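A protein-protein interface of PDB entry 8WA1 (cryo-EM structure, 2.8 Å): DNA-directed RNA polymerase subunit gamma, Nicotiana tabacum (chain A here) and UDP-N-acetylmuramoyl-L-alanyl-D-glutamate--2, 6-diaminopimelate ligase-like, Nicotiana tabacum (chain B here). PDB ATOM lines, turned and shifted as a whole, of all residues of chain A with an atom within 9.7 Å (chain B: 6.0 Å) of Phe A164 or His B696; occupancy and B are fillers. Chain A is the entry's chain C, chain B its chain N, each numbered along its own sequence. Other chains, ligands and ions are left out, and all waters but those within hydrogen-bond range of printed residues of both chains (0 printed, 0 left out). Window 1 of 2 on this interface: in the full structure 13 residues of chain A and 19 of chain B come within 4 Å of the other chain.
The backbone carbonyl oxygen of Phe A164 is in hydrogen-bond range of the backbone NH of Trp B764 (3.4 Å). O of Trp B764 sits close to N of Arg A166 (3.5 Å). The backbone carbonyl oxygen of Phe A164 lies close to the backbone carbonyl oxygen of Phe B762 (2.8 Å).
Leu B695 touches Pro A162. CB of Pro A162 touches CD2 of His B696 (3.5 Å). Phe A164 touches His B696 (CB to CE1, 3.6 Å). Pro B763 touches Phe A164. Pro B763 touches Arg A166 (CB to CB, 3.6 Å). Phe A186 touches Val B701 (CE1 to CA, 3.9 Å). Phe A186 touches Trp B764 (CZ to CH2, 3.8 Å). Phe A194 touches Ile B698. CD1 of Phe A194 touches CG1 of Val B701, 3.7 Å away. Arg A197 touches Asp B697 (NH1 to CB, 3.6 Å).
Hydrophobic or aromatic side chains of chain A that line the printed part of chain B: Pro A162, Phe A164, Phe A186 and Phe A194. Of the 16 printed residues of chain B, 8 touch a printed residue of chain A. Printed residues of chain B that touch a printed residue of chain A: Leu B695, His B696, Asp B697, Ile B698, Val B701, Phe B762, Pro B763 and Trp B764. Hydrophobic or aromatic side chains of chain B within 4 Å of the printed part of chain A: His B696, Ile B698, Val B701, Phe B762, Pro B763 and Trp B764. Along chain B the printed residues that touch a printed residue of chain A span positions 695 to 764. Among the printed residues, no Asp or Glu carboxylate lies within 4 Å of a Lys or Arg side-chain nitrogen of the other chain.
Of the printed residues of chain B, Pro A162 touches Leu B695 and His B696. Of the printed residues of chain B, Phe A194 touches Ile B698 and Val B701. Thr B648 touches none of the printed residues of chain A. Phe B694 touches none of the printed residues of chain A. Leu B695 touches just one residue of chain A: Pro A162 (3.9 Å). Of chain A, only Pro A162 and Phe A164 come within 4 Å of His B696. Printed residues of chain A within 4 Å of Val B701: Phe A186 (3.9 Å) and Phe A194 (3.7 Å). Printed residues of chain A within 4 Å of Pro B763: Phe A164 (3.7 Å) and Arg A166 (3.6 Å). Of the printed residues of chain A, Trp B764 touches Phe A164 (3.4 Å), Arg A166 (3.3 Å) and Phe A186 (3.8 Å). The nearest residue of chain A that does not touch His B696 is Arg A197 (4.4 Å).
The backbone carbonyl oxygen (O) of Leu B647 sits at hydrogen-bond distance from the backbone NH (N) of His B696, 3.0 Å away. OG1 of Thr B648 lies within hydrogen-bond range of O of Ile B698 (3.1 Å). The backbone NH (N) of Leu B695 is in hydrogen-bond range of the side-chain hydroxyl (OH) of Tyr B675 (2.7 Å).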
ATOM      1  N   ALA A 155       4.976   9.065  19.515  1.00  0.00           N
ATOM      2  CA  ALA A 155       4.071  10.070  20.068  1.00  0.00           C
ATOM      3  C   ALA A 155       3.227  10.732  18.983  1.00  0.00           C
ATOM      4  O   ALA A 155       1.996  10.783  19.088  1.00  0.00           O
ATOM      5  CB  ALA A 155       4.866  11.119  20.845  1.00  0.00           C
ATOM      6  N   ARG A 156       3.864  11.251  17.936  1.00  0.00           N
ATOM      7  CA  ARG A 156       3.157  11.992  16.890  1.00  0.00           C
ATOM      8  C   ARG A 156       3.375  11.335  15.535  1.00  0.00           C
ATOM      9  O   ARG A 156       4.396  11.593  14.872  1.00  0.00           O
ATOM     10  CB  ARG A 156       3.607  13.451  16.853  1.00  0.00           C
ATOM     11  CG  ARG A 156       2.876  14.348  17.840  1.00  0.00           C
ATOM     12  CD  ARG A 156       3.154  15.817  17.562  1.00  0.00           C
ATOM     13  NE  ARG A 156       2.276  16.691  18.333  1.00  0.00           N
ATOM     14  CZ  ARG A 156       2.323  18.019  18.298  1.00  0.00           C
ATOM     15  NH1 ARG A 156       3.210  18.633  17.528  1.00  0.00           N
ATOM     16  NH2 ARG A 156       1.483  18.733  19.034  1.00  0.00           N
ATOM     17  N   ILE A 158       1.101  11.627  12.930  1.00  0.00           N
ATOM     18  CA  ILE A 158       0.416  12.433  11.927  1.00  0.00           C
ATOM     19  C   ILE A 158       0.838  13.884  12.112  1.00  0.00           C
ATOM     20  O   ILE A 158       0.831  14.399  13.236  1.00  0.00           O
ATOM     21  CB  ILE A 158      -1.114  12.293  12.030  1.00  0.00           C
ATOM     22  CG1 ILE A 158      -1.518  10.819  11.975  1.00  0.00           C
ATOM     23  CG2 ILE A 158      -1.794  13.073  10.918  1.00  0.00           C
ATOM     24  CD1 ILE A 158      -3.004  10.588  12.139  1.00  0.00           C
ATOM     25  N   LYS A 161      -2.827  16.837  10.858  1.00  0.00           N
ATOM     26  CA  LYS A 161      -4.071  16.926  11.603  1.00  0.00           C
ATOM     27  C   LYS A 161      -3.825  17.593  12.947  1.00  0.00           C
ATOM     28  O   LYS A 161      -2.690  17.628  13.431  1.00  0.00           O
ATOM     29  CB  LYS A 161      -4.688  15.538  11.825  1.00  0.00           C
ATOM     30  N   PRO A 162      -4.870  18.139  13.566  1.00  0.00           N
ATOM     31  CA  PRO A 162      -4.693  18.770  14.880  1.00  0.00           C
ATOM     32  C   PRO A 162      -4.336  17.743  15.943  1.00  0.00           C
ATOM     33  O   PRO A 162      -4.832  16.614  15.937  1.00  0.00           O
ATOM     34  CB  PRO A 162      -6.059  19.413  15.150  1.00  0.00           C
ATOM     35  N   THR A 163      -3.460  18.145  16.863  1.00  0.00           N
ATOM     36  CA  THR A 163      -3.014  17.283  17.952  1.00  0.00           C
ATOM     37  C   THR A 163      -3.093  18.057  19.258  1.00  0.00           C
ATOM     38  O   THR A 163      -2.367  19.039  19.445  1.00  0.00           O
ATOM     39  CB  THR A 163      -1.588  16.777  17.716  1.00  0.00           C
ATOM     40  N   PHE A 164      -3.971  17.612  20.160  1.00  0.00           N
ATOM     41  CA  PHE A 164      -4.109  18.279  21.450  1.00  0.00           C
ATOM     42  C   PHE A 164      -2.926  17.965  22.359  1.00  0.00           C
ATOM     43  O   PHE A 164      -2.377  18.859  23.012  1.00  0.00           O
ATOM     44  CB  PHE A 164      -5.425  17.870  22.114  1.00  0.00           C
ATOM     45  N   LEU A 165      -2.521  16.699  22.415  1.00  0.00           N
ATOM     46  CA  LEU A 165      -1.408  16.297  23.261  1.00  0.00           C
ATOM     47  C   LEU A 165      -0.092  16.836  22.714  1.00  0.00           C
ATOM     48  O   LEU A 165       0.143  16.852  21.502  1.00  0.00           O
ATOM     49  CB  LEU A 165      -1.342  14.774  23.374  1.00  0.00           C
ATOM     50  N   ARG A 166       0.775  17.276  23.627  1.00  0.00           N
ATOM     51  CA  ARG A 166       2.054  17.876  23.268  1.00  0.00           C
ATOM     52  C   ARG A 166       3.239  16.990  23.640  1.00  0.00           C
ATOM     53  O   ARG A 166       4.271  17.500  24.086  1.00  0.00           O
ATOM     54  CB  ARG A 166       2.197  19.249  23.928  1.00  0.00           C
ATOM     55  N   LEU A 167       3.107  15.672  23.471  1.00  0.00           N
ATOM     56  CA  LEU A 167       4.218  14.772  23.764  1.00  0.00           C
ATOM     57  C   LEU A 167       5.407  15.059  22.855  1.00  0.00           C
ATOM     58  O   LEU A 167       6.503  15.381  23.330  1.00  0.00           O
ATOM     59  CB  LEU A 167       3.766  13.318  23.624  1.00  0.00           C
ATOM     60  N   ARG A 168       5.202  14.957  21.539  1.00  0.00           N
ATOM     61  CA  ARG A 168       6.221  15.248  20.536  1.00  0.00           C
ATOM     62  C   ARG A 168       7.512  14.476  20.788  1.00  0.00           C
ATOM     63  O   ARG A 168       8.600  15.060  20.793  1.00  0.00           O
ATOM     64  CB  ARG A 168       6.510  16.751  20.488  1.00  0.00           C
ATOM     65  N   PHE A 185     -11.737  10.377  30.915  1.00  0.00           N
ATOM     66  CA  PHE A 185     -12.169  11.773  30.791  1.00  0.00           C
ATOM     67  C   PHE A 185     -12.907  11.997  29.492  1.00  0.00           C
ATOM     68  O   PHE A 185     -14.057  12.439  29.490  1.00  0.00           O
ATOM     69  CB  PHE A 185     -10.960  12.704  30.851  1.00  0.00           C
ATOM     70  CG  PHE A 185     -11.307  14.159  30.750  1.00  0.00           C
ATOM     71  CD1 PHE A 185     -11.867  14.823  31.825  1.00  0.00           C
ATOM     72  CD2 PHE A 185     -11.055  14.866  29.587  1.00  0.00           C
ATOM     73  CE1 PHE A 185     -12.179  16.164  31.740  1.00  0.00           C
ATOM     74  CE2 PHE A 185     -11.364  16.208  29.498  1.00  0.00           C
ATOM     75  CZ  PHE A 185     -11.930  16.857  30.574  1.00  0.00           C
ATOM     76  N   PHE A 186     -12.248  11.706  28.383  1.00  0.00           N
ATOM     77  CA  PHE A 186     -12.886  11.844  27.086  1.00  0.00           C
ATOM     78  C   PHE A 186     -13.882  10.715  26.914  1.00  0.00           C
ATOM     79  O   PHE A 186     -13.813   9.712  27.609  1.00  0.00           O
ATOM     80  CB  PHE A 186     -11.847  11.806  25.966  1.00  0.00           C
ATOM     81  CG  PHE A 186     -10.883  12.956  25.993  1.00  0.00           C
ATOM     82  CD1 PHE A 186     -11.280  14.220  25.599  1.00  0.00           C
ATOM     83  CD2 PHE A 186      -9.573  12.772  26.400  1.00  0.00           C
ATOM     84  CE1 PHE A 186     -10.393  15.279  25.619  1.00  0.00           C
ATOM     85  CE2 PHE A 186      -8.682  13.825  26.427  1.00  0.00           C
ATOM     86  CZ  PHE A 186      -9.093  15.081  26.034  1.00  0.00           C
ATOM     87  N   GLY A 190     -14.670   8.653  21.673  1.00  0.00           N
ATOM     88  CA  GLY A 190     -13.874   9.801  21.273  1.00  0.00           C
ATOM     89  C   GLY A 190     -12.387   9.551  21.415  1.00  0.00           C
ATOM     90  O   GLY A 190     -11.605   9.974  20.568  1.00  0.00           O
ATOM     91  N   THR A 193     -11.265   7.642  18.617  1.00  0.00           N
ATOM     92  CA  THR A 193     -11.222   8.458  17.411  1.00  0.00           C
ATOM     93  C   THR A 193      -9.911   9.219  17.259  1.00  0.00           C
ATOM     94  O   THR A 193      -9.385   9.326  16.152  1.00  0.00           O
ATOM     95  CB  THR A 193     -12.388   9.459  17.364  1.00  0.00           C
ATOM     96  N   PHE A 194      -9.377   9.754  18.351  1.00  0.00           N
ATOM     97  CA  PHE A 194      -8.163  10.553  18.226  1.00  0.00           C
ATOM     98  C   PHE A 194      -6.848   9.832  18.557  1.00  0.00           C
ATOM     99  O   PHE A 194      -5.779  10.395  18.334  1.00  0.00           O
ATOM    100  CB  PHE A 194      -8.277  11.908  18.952  1.00  0.00           C
ATOM    101  CG  PHE A 194      -8.014  11.858  20.433  1.00  0.00           C
ATOM    102  CD1 PHE A 194      -9.048  11.661  21.326  1.00  0.00           C
ATOM    103  CD2 PHE A 194      -6.740  12.071  20.936  1.00  0.00           C
ATOM    104  CE1 PHE A 194      -8.815  11.637  22.687  1.00  0.00           C
ATOM    105  CE2 PHE A 194      -6.498  12.041  22.294  1.00  0.00           C
ATOM    106  CZ  PHE A 194      -7.539  11.828  23.171  1.00  0.00           C
ATOM    107  N   ARG A 195      -6.908   8.605  19.075  1.00  0.00           N
ATOM    108  CA  ARG A 195      -5.671   7.927  19.449  1.00  0.00           C
ATOM    109  C   ARG A 195      -4.738   7.778  18.255  1.00  0.00           C
ATOM    110  O   ARG A 195      -3.515   7.697  18.421  1.00  0.00           O
ATOM    111  CB  ARG A 195      -5.986   6.561  20.059  1.00  0.00           C
ATOM    112  N   ARG A 197      -4.195  10.052  15.835  1.00  0.00           N
ATOM    113  CA  ARG A 197      -3.394  11.271  15.852  1.00  0.00           C
ATOM    114  C   ARG A 197      -2.532  11.332  17.106  1.00  0.00           C
ATOM    115  O   ARG A 197      -1.515  12.035  17.139  1.00  0.00           O
ATOM    116  CB  ARG A 197      -4.306  12.494  15.759  1.00  0.00           C
ATOM    117  CG  ARG A 197      -5.304  12.419  14.615  1.00  0.00           C
ATOM    118  CD  ARG A 197      -6.348  13.521  14.707  1.00  0.00           C
ATOM    119  NE  ARG A 197      -7.382  13.373  13.688  1.00  0.00           N
ATOM    120  CZ  ARG A 197      -8.441  14.169  13.574  1.00  0.00           C
ATOM    121  NH1 ARG A 197      -8.611  15.176  14.419  1.00  0.00           N
ATOM    122  NH2 ARG A 197      -9.330  13.957  12.613  1.00  0.00           N
ATOM    123  N   GLU A 198      -2.925  10.598  18.145  1.00  0.00           N
ATOM    124  CA  GLU A 198      -2.146  10.502  19.372  1.00  0.00           C
ATOM    125  C   GLU A 198      -1.088   9.417  19.221  1.00  0.00           C
ATOM    126  O   GLU A 198      -0.804   8.973  18.104  1.00  0.00           O
ATOM    127  CB  GLU A 198      -3.051  10.210  20.571  1.00  0.00           C
ATOM    128  N   ILE A 199      -0.483   9.008  20.340  1.00  0.00           N
ATOM    129  CA  ILE A 199       0.566   7.996  20.303  1.00  0.00           C
ATOM    130  C   ILE A 199       0.044   6.726  19.644  1.00  0.00           C
ATOM    131  O   ILE A 199      -1.026   6.214  19.995  1.00  0.00           O
ATOM    132  CB  ILE A 199       1.085   7.718  21.721  1.00  0.00           C
ATOM    133  N   ILE B 646     -11.666  28.253  20.927  1.00  0.00           N
ATOM    134  CA  ILE B 646     -11.419  26.931  20.364  1.00  0.00           C
ATOM    135  C   ILE B 646     -12.473  26.676  19.297  1.00  0.00           C
ATOM    136  O   ILE B 646     -13.673  26.634  19.598  1.00  0.00           O
ATOM    137  CB  ILE B 646     -11.447  25.838  21.444  1.00  0.00           C
ATOM    138  N   LEU B 647     -12.030  26.510  18.055  1.00  0.00           N
ATOM    139  CA  LEU B 647     -12.919  26.285  16.923  1.00  0.00           C
ATOM    140  C   LEU B 647     -12.917  24.809  16.555  1.00  0.00           C
ATOM    141  O   LEU B 647     -11.852  24.207  16.381  1.00  0.00           O
ATOM    142  CB  LEU B 647     -12.495  27.129  15.719  1.00  0.00           C
ATOM    143  CG  LEU B 647     -12.717  28.637  15.823  1.00  0.00           C
ATOM    144  CD1 LEU B 647     -12.151  29.343  14.604  1.00  0.00           C
ATOM    145  CD2 LEU B 647     -14.196  28.946  15.983  1.00  0.00           C
ATOM    146  N   THR B 648     -14.111  24.231  16.439  1.00  0.00           N
ATOM    147  CA  THR B 648     -14.267  22.842  16.034  1.00  0.00           C
ATOM    148  C   THR B 648     -15.501  22.717  15.152  1.00  0.00           C
ATOM    149  O   THR B 648     -16.376  23.586  15.146  1.00  0.00           O
ATOM    150  CB  THR B 648     -14.389  21.904  17.241  1.00  0.00           C
ATOM    151  OG1 THR B 648     -14.523  20.553  16.785  1.00  0.00           O
ATOM    152  CG2 THR B 648     -15.602  22.273  18.083  1.00  0.00           C
ATOM    153  N   SER B 649     -15.599  21.655  14.369  1.00  0.00           N
ATOM    154  CA  SER B 649     -16.730  21.533  13.445  1.00  0.00           C
ATOM    155  C   SER B 649     -18.009  21.072  14.134  1.00  0.00           C
ATOM    156  O   SER B 649     -18.176  19.882  14.399  1.00  0.00           O
ATOM    157  CB  SER B 649     -16.391  20.566  12.318  1.00  0.00           C
ATOM    158  N   LEU B 661     -12.853  24.804   8.549  1.00  0.00           N
ATOM    159  CA  LEU B 661     -12.057  25.465   9.578  1.00  0.00           C
ATOM    160  C   LEU B 661     -11.040  26.416   8.962  1.00  0.00           C
ATOM    161  O   LEU B 661     -10.724  27.457   9.546  1.00  0.00           O
ATOM    162  CB  LEU B 661     -11.365  24.423  10.458  1.00  0.00           C
ATOM    163  CG  LEU B 661     -12.285  23.569  11.334  1.00  0.00           C
ATOM    164  CD1 LEU B 661     -11.484  22.551  12.132  1.00  0.00           C
ATOM    165  CD2 LEU B 661     -13.126  24.441  12.255  1.00  0.00           C
ATOM    166  N   TYR B 675      -1.407  27.206  10.943  1.00  0.00           N
ATOM    167  CA  TYR B 675      -1.793  26.767  12.259  1.00  0.00           C
ATOM    168  C   TYR B 675      -1.049  25.521  12.529  1.00  0.00           C
ATOM    169  O   TYR B 675      -0.512  25.339  13.599  1.00  0.00           O
ATOM    170  CB  TYR B 675      -3.292  26.511  12.336  1.00  0.00           C
ATOM    171  CG  TYR B 675      -3.715  26.063  13.712  1.00  0.00           C
ATOM    172  CD1 TYR B 675      -3.938  26.986  14.721  1.00  0.00           C
ATOM    173  CD2 TYR B 675      -3.863  24.717  14.009  1.00  0.00           C
ATOM    174  CE1 TYR B 675      -4.311  26.581  15.985  1.00  0.00           C
ATOM    175  CE2 TYR B 675      -4.226  24.302  15.269  1.00  0.00           C
ATOM    176  CZ  TYR B 675      -4.453  25.236  16.251  1.00  0.00           C
ATOM    177  OH  TYR B 675      -4.813  24.813  17.506  1.00  0.00           O
ATOM    178  N   PHE B 694      -7.181  28.629  19.025  1.00  0.00           N
ATOM    179  CA  PHE B 694      -6.870  27.207  18.997  1.00  0.00           C
ATOM    180  C   PHE B 694      -7.865  26.509  18.087  1.00  0.00           C
ATOM    181  O   PHE B 694      -9.015  26.938  17.976  1.00  0.00           O
ATOM    182  CB  PHE B 694      -6.917  26.599  20.406  1.00  0.00           C
ATOM    183  CG  PHE B 694      -5.774  27.015  21.290  1.00  0.00           C
ATOM    184  CD1 PHE B 694      -4.482  27.089  20.790  1.00  0.00           C
ATOM    185  CD2 PHE B 694      -5.991  27.335  22.619  1.00  0.00           C
ATOM    186  CE1 PHE B 694      -3.430  27.474  21.602  1.00  0.00           C
ATOM    187  CE2 PHE B 694      -4.942  27.720  23.436  1.00  0.00           C
ATOM    188  CZ  PHE B 694      -3.660  27.790  22.925  1.00  0.00           C
ATOM    189  N   LEU B 695      -7.412  25.441  17.432  1.00  0.00           N
ATOM    190  CA  LEU B 695      -8.212  24.743  16.435  1.00  0.00           C
ATOM    191  C   LEU B 695      -8.141  23.241  16.669  1.00  0.00           C
ATOM    192  O   LEU B 695      -7.060  22.694  16.905  1.00  0.00           O
ATOM    193  CB  LEU B 695      -7.732  25.071  15.019  1.00  0.00           C
ATOM    194  CG  LEU B 695      -8.637  24.557  13.903  1.00  0.00           C
ATOM    195  CD1 LEU B 695      -9.912  25.379  13.848  1.00  0.00           C
ATOM    196  CD2 LEU B 695      -7.920  24.575  12.567  1.00  0.00           C
ATOM    197  N   HIS B 696      -9.297  22.582  16.609  1.00  0.00           N
ATOM    198  CA  HIS B 696      -9.369  21.129  16.635  1.00  0.00           C
ATOM    199  C   HIS B 696     -10.481  20.684  15.696  1.00  0.00           C
ATOM    200  O   HIS B 696     -11.347  21.474  15.312  1.00  0.00           O
ATOM    201  CB  HIS B 696      -9.603  20.593  18.054  1.00  0.00           C
ATOM    202  CG  HIS B 696      -8.905  19.298  18.330  1.00  0.00           C
ATOM    203  ND1 HIS B 696      -8.632  18.856  19.607  1.00  0.00           N
ATOM    204  CD2 HIS B 696      -8.420  18.350  17.493  1.00  0.00           C
ATOM    205  CE1 HIS B 696      -8.008  17.694  19.545  1.00  0.00           C
ATOM    206  NE2 HIS B 696      -7.869  17.363  18.273  1.00  0.00           N
ATOM    207  N   ASP B 697     -10.442  19.408  15.315  1.00  0.00           N
ATOM    208  CA  ASP B 697     -11.388  18.869  14.350  1.00  0.00           C
ATOM    209  C   ASP B 697     -12.520  18.067  14.976  1.00  0.00           C
ATOM    210  O   ASP B 697     -13.571  17.918  14.341  1.00  0.00           O
ATOM    211  CB  ASP B 697     -10.658  17.988  13.325  1.00  0.00           C
ATOM    212  N   ILE B 698     -12.346  17.554  16.190  1.00  0.00           N
ATOM    213  CA  ILE B 698     -13.367  16.759  16.862  1.00  0.00           C
ATOM    214  C   ILE B 698     -14.073  17.637  17.885  1.00  0.00           C
ATOM    215  O   ILE B 698     -13.423  18.319  18.687  1.00  0.00           O
ATOM    216  CB  ILE B 698     -12.758  15.512  17.528  1.00  0.00           C
ATOM    217  CG1 ILE B 698     -12.069  14.634  16.481  1.00  0.00           C
ATOM    218  CG2 ILE B 698     -13.830  14.723  18.265  1.00  0.00           C
ATOM    219  CD1 ILE B 698     -11.446  13.377  17.051  1.00  0.00           C
ATOM    220  N   VAL B 701     -13.712  16.292  21.910  1.00  0.00           N
ATOM    221  CA  VAL B 701     -12.453  16.593  22.585  1.00  0.00           C
ATOM    222  C   VAL B 701     -12.279  18.097  22.740  1.00  0.00           C
ATOM    223  O   VAL B 701     -11.690  18.571  23.719  1.00  0.00           O
ATOM    224  CB  VAL B 701     -11.271  15.948  21.836  1.00  0.00           C
ATOM    225  CG1 VAL B 701     -11.496  14.450  21.694  1.00  0.00           C
ATOM    226  CG2 VAL B 701     -11.077  16.591  20.476  1.00  0.00           C
ATOM    227  N   ALA B 702     -12.810  18.876  21.795  1.00  0.00           N
ATOM    228  CA  ALA B 702     -12.741  20.328  21.919  1.00  0.00           C
ATOM    229  C   ALA B 702     -13.570  20.816  23.101  1.00  0.00           C
ATOM    230  O   ALA B 702     -13.106  21.645  23.892  1.00  0.00           O
ATOM    231  CB  ALA B 702     -13.206  20.990  20.624  1.00  0.00           C
ATOM    232  N   PHE B 762      -3.473  24.819  24.791  1.00  0.00           N
ATOM    233  CA  PHE B 762      -3.861  23.656  23.998  1.00  0.00           C
ATOM    234  C   PHE B 762      -2.773  22.589  23.923  1.00  0.00           C
ATOM    235  O   PHE B 762      -3.117  21.398  24.015  1.00  0.00           O
ATOM    236  CB  PHE B 762      -4.288  24.098  22.592  1.00  0.00           C
ATOM    237  CG  PHE B 762      -5.288  23.182  21.947  1.00  0.00           C
ATOM    238  CD1 PHE B 762      -5.869  22.149  22.666  1.00  0.00           C
ATOM    239  CD2 PHE B 762      -5.644  23.349  20.621  1.00  0.00           C
ATOM    240  CE1 PHE B 762      -6.790  21.305  22.074  1.00  0.00           C
ATOM    241  CE2 PHE B 762      -6.564  22.509  20.024  1.00  0.00           C
ATOM    242  CZ  PHE B 762      -7.136  21.486  20.751  1.00  0.00           C
ATOM    243  N   PRO B 763      -1.487  22.910  23.753  1.00  0.00           N
ATOM    244  CA  PRO B 763      -0.465  21.863  23.898  1.00  0.00           C
ATOM    245  C   PRO B 763      -0.319  21.483  25.365  1.00  0.00           C
ATOM    246  O   PRO B 763       0.296  22.209  26.149  1.00  0.00           O
ATOM    247  CB  PRO B 763       0.806  22.527  23.353  1.00  0.00           C
ATOM    248  CG  PRO B 763       0.571  23.982  23.520  1.00  0.00           C
ATOM    249  CD  PRO B 763      -0.895  24.175  23.275  1.00  0.00           C
ATOM    250  N   TRP B 764      -0.887  20.339  25.733  1.00  0.00           N
ATOM    251  CA  TRP B 764      -0.939  19.908  27.123  1.00  0.00           C
ATOM    252  C   TRP B 764       0.419  19.354  27.535  1.00  0.00           C
ATOM    253  O   TRP B 764       0.975  18.490  26.851  1.00  0.00           O
ATOM    254  CB  TRP B 764      -2.025  18.853  27.329  1.00  0.00           C
ATOM    255  CG  TRP B 764      -3.424  19.377  27.221  1.00  0.00           C
ATOM    256  CD1 TRP B 764      -3.804  20.639  26.873  1.00  0.00           C
ATOM    257  CD2 TRP B 764      -4.633  18.648  27.469  1.00  0.00           C
ATOM    258  NE1 TRP B 764      -5.174  20.743  26.886  1.00  0.00           N
ATOM    259  CE2 TRP B 764      -5.707  19.534  27.250  1.00  0.00           C
ATOM    260  CE3 TRP B 764      -4.912  17.334  27.855  1.00  0.00           C
ATOM    261  CZ2 TRP B 764      -7.036  19.148  27.402  1.00  0.00           C
ATOM    262  CZ3 TRP B 764      -6.231  16.953  28.007  1.00  0.00           C
ATOM    263  CH2 TRP B 764      -7.277  17.858  27.782  1.00  0.00           C
